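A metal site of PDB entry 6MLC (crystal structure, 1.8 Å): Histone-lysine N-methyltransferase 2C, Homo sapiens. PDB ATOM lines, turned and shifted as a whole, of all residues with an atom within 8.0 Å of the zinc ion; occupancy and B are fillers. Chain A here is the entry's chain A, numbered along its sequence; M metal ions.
Four residues have an atom within 4 Å of the zinc ion: Cys 35, Cys 38, His 59 and Cys 62.
The zinc ion is bound by a ring nitrogen (ND1) of His 59 (2.2 Å), the side-chain sulfur of Cys 62 (2.2 Å), the side-chain sulfur of Cys 38 (2.3 Å) and the side-chain sulfur of Cys 35 (2.3 Å).
NE2 of His 59 is in hydrogen-bond range of OD2 of Asp 46 (2.7 Å).
SG of Cys 35 sits close to N of Val 37.
N of Cys 35 is in hydrogen-bond range of O of Arg 40 (3.0 Å).
N of Arg 40 sits close to SG of Cys 38 (3.6 Å).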
ATOM      1  N   SER A  34     -17.216  15.053  22.846  1.00  0.00           N
ATOM      2  CA  SER A  34     -16.496  13.852  22.355  1.00  0.00           C
ATOM      3  C   SER A  34     -15.061  13.837  22.893  1.00  0.00           C
ATOM      4  O   SER A  34     -14.451  14.919  23.055  1.00  0.00           O
ATOM      5  CB  SER A  34     -16.589  13.752  20.848  1.00  0.00           C
ATOM      6  OG  SER A  34     -15.938  14.841  20.213  1.00  0.00           O
ATOM      7  N   CYS A  35     -14.537  12.634  23.123  1.00  0.00           N
ATOM      8  CA  CYS A  35     -13.156  12.399  23.664  1.00  0.00           C
ATOM      9  C   CYS A  35     -12.115  12.738  22.596  1.00  0.00           C
ATOM     10  O   CYS A  35     -12.224  12.287  21.444  1.00  0.00           O
ATOM     11  CB  CYS A  35     -13.003  10.973  24.129  1.00  0.00           C
ATOM     12  SG  CYS A  35     -11.368  10.599  24.831  1.00  0.00           S
ATOM     13  N   PRO A  36     -11.106  13.583  22.930  1.00  0.00           N
ATOM     14  CA  PRO A  36     -10.014  13.887  22.007  1.00  0.00           C
ATOM     15  C   PRO A  36      -8.994  12.736  21.859  1.00  0.00           C
ATOM     16  O   PRO A  36      -8.132  12.864  21.022  1.00  0.00           O
ATOM     17  CB  PRO A  36      -9.346  15.136  22.646  1.00  0.00           C
ATOM     18  CG  PRO A  36      -9.634  14.990  24.120  1.00  0.00           C
ATOM     19  CD  PRO A  36     -11.011  14.357  24.175  1.00  0.00           C
ATOM     20  N   VAL A  37      -9.112  11.667  22.640  1.00  0.00           N
ATOM     21  CA  VAL A  37      -8.230  10.476  22.506  1.00  0.00           C
ATOM     22  C   VAL A  37      -8.855   9.485  21.519  1.00  0.00           C
ATOM     23  O   VAL A  37      -8.186   9.143  20.527  1.00  0.00           O
ATOM     24  CB  VAL A  37      -7.917   9.798  23.856  1.00  0.00           C
ATOM     25  CG1 VAL A  37      -6.919   8.653  23.665  1.00  0.00           C
ATOM     26  CG2 VAL A  37      -7.421  10.794  24.902  1.00  0.00           C
ATOM     27  N   CYS A  38     -10.082   9.045  21.776  1.00  0.00           N
ATOM     28  CA  CYS A  38     -10.709   7.900  21.041  1.00  0.00           C
ATOM     29  C   CYS A  38     -11.707   8.403  19.995  1.00  0.00           C
ATOM     30  O   CYS A  38     -12.071   7.623  19.070  1.00  0.00           O
ATOM     31  CB  CYS A  38     -11.353   6.949  22.041  1.00  0.00           C
ATOM     32  SG  CYS A  38     -12.797   7.658  22.867  1.00  0.00           S
ATOM     33  N   TYR A  39     -12.107   9.677  20.087  1.00  0.00           N
ATOM     34  CA  TYR A  39     -13.012  10.379  19.128  1.00  0.00           C
ATOM     35  C   TYR A  39     -14.423   9.777  19.204  1.00  0.00           C
ATOM     36  O   TYR A  39     -15.192   9.979  18.271  1.00  0.00           O
ATOM     37  CB  TYR A  39     -12.389  10.358  17.733  1.00  0.00           C
ATOM     38  CG  TYR A  39     -11.146  11.218  17.663  1.00  0.00           C
ATOM     39  CD1 TYR A  39     -11.242  12.590  17.825  1.00  0.00           C
ATOM     40  CD2 TYR A  39      -9.883  10.667  17.535  1.00  0.00           C
ATOM     41  CE1 TYR A  39     -10.119  13.387  17.849  1.00  0.00           C
ATOM     42  CE2 TYR A  39      -8.740  11.462  17.524  1.00  0.00           C
ATOM     43  CZ  TYR A  39      -8.861  12.826  17.701  1.00  0.00           C
ATOM     44  OH  TYR A  39      -7.779  13.659  17.652  1.00  0.00           O
ATOM     45  N   ARG A  40     -14.793   9.207  20.341  1.00  0.00           N
ATOM     46  CA  ARG A  40     -16.177   8.749  20.620  1.00  0.00           C
ATOM     47  C   ARG A  40     -16.953   9.845  21.347  1.00  0.00           C
ATOM     48  O   ARG A  40     -16.411  10.444  22.290  1.00  0.00           O
ATOM     49  CB  ARG A  40     -16.144   7.457  21.432  1.00  0.00           C
ATOM     50  CG  ARG A  40     -15.520   6.280  20.691  1.00  0.00           C
ATOM     51  CD  ARG A  40     -16.378   5.836  19.534  1.00  0.00           C
ATOM     52  NE  ARG A  40     -16.412   4.389  19.410  1.00  0.00           N
ATOM     53  CZ  ARG A  40     -17.359   3.686  18.796  1.00  0.00           C
ATOM     54  NH1 ARG A  40     -18.397   4.296  18.241  1.00  0.00           N
ATOM     55  NH2 ARG A  40     -17.272   2.376  18.745  1.00  0.00           N
ATOM     56  N   ASN A  41     -18.203  10.072  20.941  1.00  0.00           N
ATOM     57  CA  ASN A  41     -19.176  10.870  21.728  1.00  0.00           C
ATOM     58  C   ASN A  41     -19.199  10.283  23.137  1.00  0.00           C
ATOM     59  O   ASN A  41     -19.167   9.054  23.252  1.00  0.00           O
ATOM     60  CB  ASN A  41     -20.587  10.834  21.148  1.00  0.00           C
ATOM     61  CG  ASN A  41     -20.684  11.501  19.800  1.00  0.00           C
ATOM     62  OD1 ASN A  41     -19.843  12.302  19.425  1.00  0.00           O
ATOM     63  ND2 ASN A  41     -21.733  11.191  19.074  1.00  0.00           N
ATOM     64  N   TYR A  42     -19.235  11.103  24.167  1.00  0.00           N
ATOM     65  CA  TYR A  42     -19.362  10.615  25.557  1.00  0.00           C
ATOM     66  C   TYR A  42     -20.727   9.938  25.688  1.00  0.00           C
ATOM     67  O   TYR A  42     -21.696  10.390  25.054  1.00  0.00           O
ATOM     68  CB  TYR A  42     -19.220  11.726  26.578  1.00  0.00           C
ATOM     69  CG  TYR A  42     -17.880  12.397  26.597  1.00  0.00           C
ATOM     70  CD1 TYR A  42     -16.706  11.671  26.726  1.00  0.00           C
ATOM     71  CD2 TYR A  42     -17.778  13.766  26.424  1.00  0.00           C
ATOM     72  CE1 TYR A  42     -15.472  12.293  26.717  1.00  0.00           C
ATOM     73  CE2 TYR A  42     -16.551  14.403  26.419  1.00  0.00           C
ATOM     74  CZ  TYR A  42     -15.394  13.665  26.567  1.00  0.00           C
ATOM     75  OH  TYR A  42     -14.197  14.292  26.519  1.00  0.00           O
ATOM     76  N   ASP A  46     -20.082   8.523  31.574  1.00  0.00           N
ATOM     77  CA  ASP A  46     -18.626   8.453  31.258  1.00  0.00           C
ATOM     78  C   ASP A  46     -17.862   9.296  32.294  1.00  0.00           C
ATOM     79  O   ASP A  46     -18.256  10.459  32.548  1.00  0.00           O
ATOM     80  CB  ASP A  46     -18.326   8.914  29.824  1.00  0.00           C
ATOM     81  CG  ASP A  46     -18.545   7.830  28.785  1.00  0.00           C
ATOM     82  OD1 ASP A  46     -18.940   6.687  29.205  1.00  0.00           O
ATOM     83  OD2 ASP A  46     -18.383   8.126  27.572  1.00  0.00           O
ATOM     84  N   LEU A  47     -16.826   8.703  32.888  1.00  0.00           N
ATOM     85  CA  LEU A  47     -15.888   9.355  33.830  1.00  0.00           C
ATOM     86  C   LEU A  47     -14.901  10.165  32.983  1.00  0.00           C
ATOM     87  O   LEU A  47     -14.151   9.529  32.198  1.00  0.00           O
ATOM     88  CB  LEU A  47     -15.131   8.280  34.611  1.00  0.00           C
ATOM     89  CG  LEU A  47     -14.942   8.477  36.115  1.00  0.00           C
ATOM     90  CD1 LEU A  47     -13.715   7.714  36.582  1.00  0.00           C
ATOM     91  CD2 LEU A  47     -14.882   9.940  36.515  1.00  0.00           C
ATOM     92  N   ILE A  48     -14.854  11.473  33.145  1.00  0.00           N
ATOM     93  CA  ILE A  48     -13.961  12.334  32.310  1.00  0.00           C
ATOM     94  C   ILE A  48     -13.179  13.257  33.226  1.00  0.00           C
ATOM     95  O   ILE A  48     -13.639  13.528  34.360  1.00  0.00           O
ATOM     96  CB  ILE A  48     -14.771  13.110  31.243  1.00  0.00           C
ATOM     97  CG1 ILE A  48     -15.876  13.982  31.862  1.00  0.00           C
ATOM     98  CG2 ILE A  48     -15.307  12.154  30.169  1.00  0.00           C
ATOM     99  CD1 ILE A  48     -16.506  14.968  30.891  1.00  0.00           C
ATOM    100  N   TRP A  57     -11.264  18.153  28.129  1.00  0.00           N
ATOM    101  CA  TRP A  57     -11.831  16.958  28.811  1.00  0.00           C
ATOM    102  C   TRP A  57     -11.504  15.725  28.000  1.00  0.00           C
ATOM    103  O   TRP A  57     -11.439  15.816  26.723  1.00  0.00           O
ATOM    104  CB  TRP A  57     -13.328  17.139  29.006  1.00  0.00           C
ATOM    105  CG  TRP A  57     -13.679  18.231  29.966  1.00  0.00           C
ATOM    106  CD1 TRP A  57     -13.896  19.548  29.656  1.00  0.00           C
ATOM    107  CD2 TRP A  57     -13.797  18.139  31.402  1.00  0.00           C
ATOM    108  NE1 TRP A  57     -14.172  20.266  30.789  1.00  0.00           N
ATOM    109  CE2 TRP A  57     -14.126  19.439  31.875  1.00  0.00           C
ATOM    110  CE3 TRP A  57     -13.685  17.088  32.316  1.00  0.00           C
ATOM    111  CZ2 TRP A  57     -14.338  19.705  33.225  1.00  0.00           C
ATOM    112  CZ3 TRP A  57     -13.884  17.369  33.655  1.00  0.00           C
ATOM    113  CH2 TRP A  57     -14.219  18.656  34.085  1.00  0.00           C
ATOM    114  N   MET A  58     -11.421  14.582  28.649  1.00  0.00           N
ATOM    115  CA  MET A  58     -11.253  13.299  27.969  1.00  0.00           C
ATOM    116  C   MET A  58     -11.669  12.164  28.896  1.00  0.00           C
ATOM    117  O   MET A  58     -11.694  12.354  30.134  1.00  0.00           O
ATOM    118  CB  MET A  58      -9.809  13.118  27.515  1.00  0.00           C
ATOM    119  CG  MET A  58      -8.799  13.072  28.655  1.00  0.00           C
ATOM    120  SD  MET A  58      -7.113  13.507  28.148  1.00  0.00           S
ATOM    121  CE  MET A  58      -7.239  15.256  27.771  1.00  0.00           C
ATOM    122  N   HIS A  59     -11.933  10.995  28.330  1.00  0.00           N
ATOM    123  CA  HIS A  59     -12.212   9.761  29.108  1.00  0.00           C
ATOM    124  C   HIS A  59     -11.024   9.463  30.030  1.00  0.00           C
ATOM    125  O   HIS A  59      -9.888   9.358  29.527  1.00  0.00           O
ATOM    126  CB  HIS A  59     -12.383   8.531  28.215  1.00  0.00           C
ATOM    127  CG  HIS A  59     -13.671   8.448  27.487  1.00  0.00           C
ATOM    128  ND1 HIS A  59     -13.717   8.315  26.112  1.00  0.00           N
ATOM    129  CD2 HIS A  59     -14.949   8.415  27.909  1.00  0.00           C
ATOM    130  CE1 HIS A  59     -14.971   8.205  25.722  1.00  0.00           C
ATOM    131  NE2 HIS A  59     -15.742   8.238  26.816  1.00  0.00           N
ATOM    132  N   ALA A  60     -11.301   9.199  31.298  1.00  0.00           N
ATOM    133  CA  ALA A  60     -10.332   8.609  32.236  1.00  0.00           C
ATOM    134  C   ALA A  60      -9.736   7.325  31.631  1.00  0.00           C
ATOM    135  O   ALA A  60      -8.476   7.178  31.666  1.00  0.00           O
ATOM    136  CB  ALA A  60     -10.967   8.346  33.571  1.00  0.00           C
ATOM    137  N   VAL A  61     -10.567   6.421  31.084  1.00  0.00           N
ATOM    138  CA  VAL A  61     -10.052   5.100  30.592  1.00  0.00           C
ATOM    139  C   VAL A  61      -9.083   5.318  29.420  1.00  0.00           C
ATOM    140  O   VAL A  61      -8.142   4.500  29.246  1.00  0.00           O
ATOM    141  CB  VAL A  61     -11.177   4.110  30.234  1.00  0.00           C
ATOM    142  CG1 VAL A  61     -12.027   3.812  31.458  1.00  0.00           C
ATOM    143  CG2 VAL A  61     -12.071   4.581  29.084  1.00  0.00           C
ATOM    144  N   CYS A  62      -9.234   6.406  28.670  1.00  0.00           N
ATOM    145  CA  CYS A  62      -8.373   6.728  27.510  1.00  0.00           C
ATOM    146  C   CYS A  62      -7.019   7.317  27.990  1.00  0.00           C
ATOM    147  O   CYS A  62      -6.166   7.563  27.156  1.00  0.00           O
ATOM    148  CB  CYS A  62      -9.088   7.657  26.534  1.00  0.00           C
ATOM    149  SG  CYS A  62     -10.429   6.833  25.616  1.00  0.00           S
ATOM    150  N   GLN A  63      -6.836   7.450  29.296  1.00  0.00           N
ATOM    151  CA  GLN A  63      -5.562   7.871  29.933  1.00  0.00           C
ATOM    152  C   GLN A  63      -5.134   6.837  30.960  1.00  0.00           C
ATOM    153  O   GLN A  63      -4.302   7.170  31.804  1.00  0.00           O
ATOM    154  CB  GLN A  63      -5.708   9.263  30.575  1.00  0.00           C
ATOM    155  CG  GLN A  63      -5.964  10.367  29.563  1.00  0.00           C
ATOM    156  CD  GLN A  63      -4.707  10.738  28.798  1.00  0.00           C
ATOM    157  OE1 GLN A  63      -3.807  11.378  29.334  1.00  0.00           O
ATOM    158  NE2 GLN A  63      -4.618  10.297  27.544  1.00  0.00           N
HETATM  159 ZN    ZN M   1     -11.931   8.339  24.910  1.00  0.00          ZN
